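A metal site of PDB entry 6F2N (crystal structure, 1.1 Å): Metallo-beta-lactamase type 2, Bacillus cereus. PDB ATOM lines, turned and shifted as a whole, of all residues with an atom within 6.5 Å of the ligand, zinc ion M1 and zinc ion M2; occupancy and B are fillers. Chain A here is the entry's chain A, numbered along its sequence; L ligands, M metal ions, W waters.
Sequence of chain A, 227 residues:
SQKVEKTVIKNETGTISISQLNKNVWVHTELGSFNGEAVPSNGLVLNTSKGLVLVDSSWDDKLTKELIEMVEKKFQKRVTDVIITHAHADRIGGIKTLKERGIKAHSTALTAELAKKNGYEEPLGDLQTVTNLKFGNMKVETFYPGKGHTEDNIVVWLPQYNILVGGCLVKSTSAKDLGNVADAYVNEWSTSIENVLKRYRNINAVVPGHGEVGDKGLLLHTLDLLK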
ATOM      1  N   VAL A  39      -9.917 -24.620   3.362  1.00  0.00           N
ATOM      2  CA  VAL A  39     -11.357 -24.724   3.573  1.00  0.00           C
ATOM      3  C   VAL A  39     -11.956 -23.580   2.779  1.00  0.00           C
ATOM      4  O   VAL A  39     -11.763 -22.408   3.164  1.00  0.00           O
ATOM      5  CB  VAL A  39     -11.738 -24.619   5.067  1.00  0.00           C
ATOM      6  CG1 VAL A  39     -13.298 -24.688   5.235  1.00  0.00           C
ATOM      7  CG2 VAL A  39     -11.057 -25.690   5.907  1.00  0.00           C
ATOM      8  N   PRO A  40     -12.712 -23.853   1.714  1.00  0.00           N
ATOM      9  CA  PRO A  40     -13.385 -22.765   0.991  1.00  0.00           C
ATOM     10  C   PRO A  40     -14.616 -22.286   1.695  1.00  0.00           C
ATOM     11  O   PRO A  40     -15.249 -23.019   2.443  1.00  0.00           O
ATOM     12  CB  PRO A  40     -13.778 -23.425  -0.329  1.00  0.00           C
ATOM     13  CG  PRO A  40     -14.125 -24.743   0.081  1.00  0.00           C
ATOM     14  CD  PRO A  40     -13.042 -25.132   1.107  1.00  0.00           C
ATOM     15  N   SER A  41     -14.956 -21.026   1.432  1.00  0.00           N
ATOM     16  CA  SER A  41     -16.185 -20.479   1.945  1.00  0.00           C
ATOM     17  C   SER A  41     -16.764 -19.503   0.948  1.00  0.00           C
ATOM     18  O   SER A  41     -16.032 -18.923   0.134  1.00  0.00           O
ATOM     19  CB  SER A  41     -15.949 -19.777   3.273  1.00  0.00           C
ATOM     20  OG  SER A  41     -15.017 -18.728   3.091  1.00  0.00           O
ATOM     21  N   TRP A  59     -12.312 -15.025   6.068  1.00  0.00           N
ATOM     22  CA  TRP A  59     -11.683 -15.644   7.228  1.00  0.00           C
ATOM     23  C   TRP A  59     -10.852 -14.703   8.053  1.00  0.00           C
ATOM     24  O   TRP A  59     -10.670 -14.979   9.250  1.00  0.00           O
ATOM     25  CB  TRP A  59     -10.799 -16.807   6.758  1.00  0.00           C
ATOM     26  CG  TRP A  59     -11.508 -17.889   6.066  1.00  0.00           C
ATOM     27  CD1 TRP A  59     -11.741 -18.007   4.697  1.00  0.00           C
ATOM     28  CD2 TRP A  59     -12.118 -19.028   6.684  1.00  0.00           C
ATOM     29  NE1 TRP A  59     -12.410 -19.216   4.455  1.00  0.00           N
ATOM     30  CE2 TRP A  59     -12.647 -19.848   5.652  1.00  0.00           C
ATOM     31  CE3 TRP A  59     -12.198 -19.494   8.037  1.00  0.00           C
ATOM     32  CZ2 TRP A  59     -13.258 -21.081   5.901  1.00  0.00           C
ATOM     33  CZ3 TRP A  59     -12.826 -20.698   8.262  1.00  0.00           C
ATOM     34  CH2 TRP A  59     -13.305 -21.509   7.203  1.00  0.00           C
ATOM     35  N   HIS A  86     -23.315 -14.733  10.676  1.00  0.00           N
ATOM     36  CA  HIS A  86     -23.147 -15.250  12.043  1.00  0.00           C
ATOM     37  C   HIS A  86     -21.734 -14.867  12.483  1.00  0.00           C
ATOM     38  O   HIS A  86     -20.963 -14.292  11.748  1.00  0.00           O
ATOM     39  CB  HIS A  86     -23.470 -16.730  12.244  1.00  0.00           C
ATOM     40  CG  HIS A  86     -22.553 -17.701  11.591  1.00  0.00           C
ATOM     41  ND1 HIS A  86     -22.682 -18.081  10.277  1.00  0.00           N
ATOM     42  CD2 HIS A  86     -21.595 -18.527  12.107  1.00  0.00           C
ATOM     43  CE1 HIS A  86     -21.759 -18.985  10.030  1.00  0.00           C
ATOM     44  NE2 HIS A  86     -21.113 -19.312  11.108  1.00  0.00           N
ATOM     45  N   ALA A  87     -21.425 -15.152  13.738  1.00  0.00           N
ATOM     46  CA  ALA A  87     -20.207 -14.659  14.412  1.00  0.00           C
ATOM     47  C   ALA A  87     -19.003 -15.606  14.379  1.00  0.00           C
ATOM     48  O   ALA A  87     -17.991 -15.236  15.012  1.00  0.00           O
ATOM     49  CB  ALA A  87     -20.511 -14.207  15.836  1.00  0.00           C
ATOM     50  N   HIS A  88     -18.924 -16.522  13.476  1.00  0.00           N
ATOM     51  CA  HIS A  88     -17.709 -17.337  13.262  1.00  0.00           C
ATOM     52  C   HIS A  88     -16.727 -16.614  12.268  1.00  0.00           C
ATOM     53  O   HIS A  88     -17.096 -15.805  11.469  1.00  0.00           O
ATOM     54  CB  HIS A  88     -18.060 -18.724  12.684  1.00  0.00           C
ATOM     55  CG  HIS A  88     -18.639 -19.712  13.672  1.00  0.00           C
ATOM     56  ND1 HIS A  88     -19.369 -20.805  13.271  1.00  0.00           N
ATOM     57  CD2 HIS A  88     -18.517 -19.810  15.014  1.00  0.00           C
ATOM     58  CE1 HIS A  88     -19.691 -21.533  14.335  1.00  0.00           C
ATOM     59  NE2 HIS A  88     -19.164 -20.954  15.403  1.00  0.00           N
ATOM     60  N   ALA A  89     -15.474 -17.074  12.287  1.00  0.00           N
ATOM     61  CA  ALA A  89     -14.395 -16.412  11.546  1.00  0.00           C
ATOM     62  C   ALA A  89     -14.627 -16.345  10.032  1.00  0.00           C
ATOM     63  O   ALA A  89     -14.206 -15.366   9.389  1.00  0.00           O
ATOM     64  CB  ALA A  89     -13.064 -17.083  11.817  1.00  0.00           C
ATOM     65  N   ASP A  90     -15.162 -17.379   9.423  1.00  0.00           N
ATOM     66  CA  ASP A  90     -15.403 -17.392   7.992  1.00  0.00           C
ATOM     67  C   ASP A  90     -16.272 -16.253   7.580  1.00  0.00           C
ATOM     68  O   ASP A  90     -16.174 -15.776   6.454  1.00  0.00           O
ATOM     69  CB  ASP A  90     -15.909 -18.723   7.437  1.00  0.00           C
ATOM     70  CG  ASP A  90     -17.231 -19.197   8.033  1.00  0.00           C
ATOM     71  OD1 ASP A  90     -17.555 -18.903   9.197  1.00  0.00           O
ATOM     72  OD2 ASP A  90     -17.922 -19.978   7.331  1.00  0.00           O
ATOM     73  N   ARG A  91     -17.223 -15.872   8.454  1.00  0.00           N
ATOM     74  CA  ARG A  91     -18.128 -14.771   8.171  1.00  0.00           C
ATOM     75  C   ARG A  91     -17.667 -13.384   8.604  1.00  0.00           C
ATOM     76  O   ARG A  91     -17.865 -12.400   7.899  1.00  0.00           O
ATOM     77  CB  ARG A  91     -19.453 -14.995   8.909  1.00  0.00           C
ATOM     78  CG  ARG A  91     -20.057 -16.386   8.803  1.00  0.00           C
ATOM     79  CD  ARG A  91     -20.601 -16.670   7.417  1.00  0.00           C
ATOM     80  NE  ARG A  91     -19.770 -17.638   6.705  1.00  0.00           N
ATOM     81  CZ  ARG A  91     -19.828 -17.870   5.401  1.00  0.00           C
ATOM     82  NH1 ARG A  91     -20.673 -17.179   4.643  1.00  0.00           N
ATOM     83  NH2 ARG A  91     -19.035 -18.773   4.850  1.00  0.00           N
ATOM     84  N   HIS A 149     -26.976 -24.049  12.720  1.00  0.00           N
ATOM     85  CA  HIS A 149     -25.532 -24.144  12.720  1.00  0.00           C
ATOM     86  C   HIS A 149     -24.923 -23.400  13.887  1.00  0.00           C
ATOM     87  O   HIS A 149     -23.957 -23.841  14.494  1.00  0.00           O
ATOM     88  CB  HIS A 149     -25.004 -23.639  11.385  1.00  0.00           C
ATOM     89  CG  HIS A 149     -23.551 -23.364  11.383  1.00  0.00           C
ATOM     90  ND1 HIS A 149     -22.585 -24.357  11.392  1.00  0.00           N
ATOM     91  CD2 HIS A 149     -22.897 -22.200  11.427  1.00  0.00           C
ATOM     92  CE1 HIS A 149     -21.393 -23.774  11.395  1.00  0.00           C
ATOM     93  NE2 HIS A 149     -21.540 -22.430  11.422  1.00  0.00           N
ATOM     94  N   THR A 150     -25.458 -22.214  14.176  1.00  0.00           N
ATOM     95  CA  THR A 150     -25.195 -21.441  15.361  1.00  0.00           C
ATOM     96  C   THR A 150     -26.508 -20.930  15.914  1.00  0.00           C
ATOM     97  O   THR A 150     -27.547 -20.977  15.272  1.00  0.00           O
ATOM     98  CB  THR A 150     -24.232 -20.294  15.130  1.00  0.00           C
ATOM     99  OG1 THR A 150     -24.824 -19.448  14.141  1.00  0.00           O
ATOM    100  CG2 THR A 150     -22.853 -20.781  14.733  1.00  0.00           C
ATOM    101  N   GLY A 167     -26.033 -19.450   3.829  1.00  0.00           N
ATOM    102  CA  GLY A 167     -24.982 -19.410   4.768  1.00  0.00           C
ATOM    103  C   GLY A 167     -24.726 -20.784   5.364  1.00  0.00           C
ATOM    104  O   GLY A 167     -25.062 -21.811   4.792  1.00  0.00           O
ATOM    105  N   CYS A 168     -24.144 -20.801   6.555  1.00  0.00           N
ATOM    106  CA  CYS A 168     -23.692 -22.032   7.097  1.00  0.00           C
ATOM    107  C   CYS A 168     -24.801 -22.869   7.727  1.00  0.00           C
ATOM    108  O   CYS A 168     -24.574 -24.036   8.029  1.00  0.00           O
ATOM    109  CB  CYS A 168     -22.522 -21.789   7.992  1.00  0.00           C
ATOM    110  SG  CYS A 168     -21.204 -20.774   7.117  1.00  0.00           S
ATOM    111  N   LEU A 169     -25.994 -22.316   7.793  1.00  0.00           N
ATOM    112  CA  LEU A 169     -27.216 -23.094   8.081  1.00  0.00           C
ATOM    113  C   LEU A 169     -27.471 -24.157   7.027  1.00  0.00           C
ATOM    114  O   LEU A 169     -28.155 -25.176   7.312  1.00  0.00           O
ATOM    115  CB  LEU A 169     -28.401 -22.099   8.097  1.00  0.00           C
ATOM    116  CG  LEU A 169     -29.734 -22.655   8.472  1.00  0.00           C
ATOM    117  CD1 LEU A 169     -29.866 -22.976   9.984  1.00  0.00           C
ATOM    118  CD2 LEU A 169     -30.849 -21.656   8.091  1.00  0.00           C
ATOM    119  N   LYS A 171     -26.099 -26.850   4.170  1.00  0.00           N
ATOM    120  CA  LYS A 171     -24.974 -27.645   3.711  1.00  0.00           C
ATOM    121  C   LYS A 171     -25.036 -27.919   2.218  1.00  0.00           C
ATOM    122  O   LYS A 171     -26.119 -28.115   1.657  1.00  0.00           O
ATOM    123  CB  LYS A 171     -25.001 -28.972   4.487  1.00  0.00           C
ATOM    124  CG  LYS A 171     -24.844 -28.783   6.002  1.00  0.00           C
ATOM    125  CD  LYS A 171     -23.444 -28.208   6.344  1.00  0.00           C
ATOM    126  CE  LYS A 171     -23.088 -28.089   7.749  1.00  0.00           C
ATOM    127  NZ  LYS A 171     -21.659 -27.682   7.955  1.00  0.00           N
ATOM    128  N   LEU A 178     -22.589 -32.820   9.327  1.00  0.00           N
ATOM    129  CA  LEU A 178     -22.898 -31.455   9.713  1.00  0.00           C
ATOM    130  C   LEU A 178     -21.676 -30.609  10.002  1.00  0.00           C
ATOM    131  O   LEU A 178     -21.824 -29.435  10.254  1.00  0.00           O
ATOM    132  CB  LEU A 178     -23.784 -31.492  10.940  1.00  0.00           C
ATOM    133  CG  LEU A 178     -25.165 -32.167  10.734  1.00  0.00           C
ATOM    134  CD1 LEU A 178     -25.822 -32.422  12.067  1.00  0.00           C
ATOM    135  CD2 LEU A 178     -26.030 -31.276   9.806  1.00  0.00           C
ATOM    136  N   GLY A 179     -20.504 -31.184  10.011  1.00  0.00           N
ATOM    137  CA  GLY A 179     -19.331 -30.408  10.260  1.00  0.00           C
ATOM    138  C   GLY A 179     -19.161 -30.047  11.732  1.00  0.00           C
ATOM    139  O   GLY A 179     -19.527 -30.792  12.644  1.00  0.00           O
ATOM    140  N   ASN A 180     -18.634 -28.868  11.991  1.00  0.00           N
ATOM    141  CA  ASN A 180     -18.359 -28.443  13.355  1.00  0.00           C
ATOM    142  C   ASN A 180     -19.678 -28.028  14.005  1.00  0.00           C
ATOM    143  O   ASN A 180     -20.297 -27.024  13.613  1.00  0.00           O
ATOM    144  CB  ASN A 180     -17.326 -27.321  13.416  1.00  0.00           C
ATOM    145  CG  ASN A 180     -16.844 -27.043  14.841  1.00  0.00           C
ATOM    146  OD1 ASN A 180     -17.629 -26.973  15.751  1.00  0.00           O
ATOM    147  ND2 ASN A 180     -15.520 -26.839  15.008  1.00  0.00           N
ATOM    148  N   VAL A 181     -20.074 -28.779  15.018  1.00  0.00           N
ATOM    149  CA  VAL A 181     -21.339 -28.624  15.714  1.00  0.00           C
ATOM    150  C   VAL A 181     -21.123 -28.148  17.147  1.00  0.00           C
ATOM    151  O   VAL A 181     -22.084 -28.098  17.924  1.00  0.00           O
ATOM    152  CB  VAL A 181     -22.231 -29.872  15.639  1.00  0.00           C
ATOM    153  CG1 VAL A 181     -22.695 -30.180  14.237  1.00  0.00           C
ATOM    154  CG2 VAL A 181     -21.481 -31.113  16.299  1.00  0.00           C
ATOM    155  N   ALA A 182     -19.931 -27.636  17.450  1.00  0.00           N
ATOM    156  CA  ALA A 182     -19.669 -27.160  18.798  1.00  0.00           C
ATOM    157  C   ALA A 182     -20.673 -26.065  19.209  1.00  0.00           C
ATOM    158  O   ALA A 182     -21.067 -25.967  20.391  1.00  0.00           O
ATOM    159  CB  ALA A 182     -18.253 -26.568  18.885  1.00  0.00           C
ATOM    160  N   ASP A 183     -21.036 -25.209  18.276  1.00  0.00           N
ATOM    161  CA  ASP A 183     -21.885 -24.077  18.544  1.00  0.00           C
ATOM    162  C   ASP A 183     -23.293 -24.268  18.017  1.00  0.00           C
ATOM    163  O   ASP A 183     -24.073 -23.304  17.983  1.00  0.00           O
ATOM    164  CB  ASP A 183     -21.229 -22.802  17.988  1.00  0.00           C
ATOM    165  CG  ASP A 183     -19.911 -22.490  18.659  1.00  0.00           C
ATOM    166  OD1 ASP A 183     -19.787 -22.681  19.870  1.00  0.00           O
ATOM    167  OD2 ASP A 183     -19.038 -22.003  17.962  1.00  0.00           O
ATOM    168  N   GLY A 209     -22.981 -21.898   2.772  1.00  0.00           N
ATOM    169  CA  GLY A 209     -21.817 -21.219   3.319  1.00  0.00           C
ATOM    170  C   GLY A 209     -20.509 -21.755   2.800  1.00  0.00           C
ATOM    171  O   GLY A 209     -19.502 -21.031   2.730  1.00  0.00           O
ATOM    172  N   HIS A 210     -20.497 -23.040   2.434  1.00  0.00           N
ATOM    173  CA  HIS A 210     -19.345 -23.732   1.897  1.00  0.00           C
ATOM    174  C   HIS A 210     -19.837 -24.668   0.788  1.00  0.00           C
ATOM    175  O   HIS A 210     -20.868 -25.325   0.949  1.00  0.00           O
ATOM    176  CB  HIS A 210     -18.592 -24.531   3.038  1.00  0.00           C
ATOM    177  CG  HIS A 210     -18.258 -23.704   4.287  1.00  0.00           C
ATOM    178  ND1 HIS A 210     -17.103 -22.983   4.467  1.00  0.00           N
ATOM    179  CD2 HIS A 210     -19.007 -23.449   5.417  1.00  0.00           C
ATOM    180  CE1 HIS A 210     -17.162 -22.303   5.597  1.00  0.00           C
ATOM    181  NE2 HIS A 210     -18.304 -22.583   6.216  1.00  0.00           N
HETATM  182  C1  LIG L   1     -17.329 -23.781  13.453  1.00  0.00           C
HETATM  183  C2  LIG L   1     -16.595 -23.196  14.451  1.00  0.00           C
HETATM  184  C3  LIG L   1     -15.458 -22.517  14.152  1.00  0.00           C
HETATM  185  C4  LIG L   1     -15.020 -22.424  12.840  1.00  0.00           C
HETATM  186  C5  LIG L   1     -15.739 -22.994  11.787  1.00  0.00           C
HETATM  187  C6  LIG L   1     -15.209 -22.907  10.362  1.00  0.00           C
HETATM  188  C7  LIG L   1     -15.035 -24.242   9.636  1.00  0.00           C
HETATM  189  C8  LIG L   1     -15.714 -24.495   8.477  1.00  0.00           C
HETATM  190  C9  LIG L   1     -15.580 -25.715   7.776  1.00  0.00           C
HETATM  191  C10 LIG L   1     -16.254 -25.986   6.553  1.00  0.00           C
HETATM  192  C11 LIG L   1     -16.103 -27.187   5.913  1.00  0.00           C
HETATM  193  C12 LIG L   1     -15.249 -28.159   6.435  1.00  0.00           C
HETATM  194  C13 LIG L   1     -18.484 -23.468  10.076  1.00  0.00           C
HETATM  195  O1  LIG L   1     -19.991 -23.617   8.332  1.00  0.00           O
HETATM  196  C14 LIG L   1     -19.291 -24.272   9.130  1.00  0.00           C
HETATM  197  C15 LIG L   1     -14.559 -27.933   7.602  1.00  0.00           C
HETATM  198  C16 LIG L   1     -14.711 -26.706   8.300  1.00  0.00           C
HETATM  199  C17 LIG L   1     -14.022 -26.431   9.504  1.00  0.00           C
HETATM  200  C18 LIG L   1     -14.192 -25.224  10.141  1.00  0.00           C
HETATM  201  C19 LIG L   1     -17.817 -24.164  11.046  1.00  0.00           C
HETATM  202  C20 LIG L   1     -16.941 -23.662  12.111  1.00  0.00           C
HETATM  203  O2  LIG L   1     -19.455 -25.532   9.215  1.00  0.00           O
HETATM  204  S1  LIG L   1     -18.380 -21.714   9.944  1.00  0.00           S
HETATM  205 ZN    ZN M   1     -19.217 -21.618   7.775  1.00  0.00          ZN
HETATM  206 ZN    ZN M   2     -20.067 -21.057  11.412  1.00  0.00          ZN
HETATM  207  O   HOH W   1     -15.287 -26.015   2.975  1.00  0.00           O
HETATM  208  O   HOH W   2     -17.879 -27.530   9.421  1.00  0.00           O
HETATM  209  O   HOH W   3     -22.080 -25.007   7.159  1.00  0.00           O
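An oxygen (O2) of the ligand is in salt-bridge range of the side-chain amino group of Lys 171, 3.3 Å away.
The side-chain amide oxygen (OD1) of Asn 180 lies within hydrogen-bond range of the backbone NH (N) of Ala 182. NE2 of His 88 sits at hydrogen-bond distance from OD2 of Asp 183 (2.8 Å). The side-chain amino group (NZ) of Lys 171 is in hydrogen-bond range of the backbone carbonyl oxygen (O) of Leu 178, 2.9 Å away. OG of Ser 41 is in hydrogen-bond range of NE1 of Trp 59, 3.0 Å away. The side-chain sulfur (SG) of Cys 168 lies close to the guanidinium group (NE) of Arg 91. The side-chain carboxylate (OD1) of Asp 90 is in salt-bridge range of the guanidinium group (NE) of Arg 91. O of Pro 40 is in hydrogen-bond range of ND1 of His 210, at 2.7 Å.
Val 39 touches the ligand. CZ3 of Trp 59 touches C6 of the ligand, at 3.9 Å. CB of Asn 180 touches C1 of the ligand, 3.5 Å away. Of the 24 residues printed, 10 come within 4 Å of the ligand.
Of the 24 residues printed, 3 come within 4 Å of zinc ion M1. The nearest printed residue that does not touch zinc ion M1 is Arg 91 (4.1 Å).
Four residues have an atom within 4 Å of zinc ion M2: His 86, His 88, Asp 90 and His 149. The nearest printed residue that does not touch zinc ion M2 is Cys 168 (4.3 Å).
Zinc ion M1 is bound by NE2 of His 210 (2.0 Å), OD2 of Asp 90 (2.1 Å), O1 of the ligand (2.2 Å), SG of Cys 168 (2.3 Å) and S1 of the ligand (2.3 Å). Zinc ion M1 has five donor atoms within binding distance.
Zinc ion M2 is bound by a ring nitrogen (ND1) of His 88 (2.0 Å), a ring nitrogen (NE2) of His 149 (2.0 Å), a ring nitrogen (NE2) of His 86 (2.1 Å) and a sulfur (S1) of the ligand (2.3 Å). Zinc ion M2 has four donor atoms within binding distance.
Water W2 lies within hydrogen-bond range of an oxygen (O2) of the ligand (2.6 Å) and the backbone NH (N) of Asn 180 (3.0 Å). Water W3 lies within hydrogen-bond range of the backbone carbonyl oxygen of Cys 168, the side-chain amino group of Lys 171 and an oxygen (O2) of the ligand.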
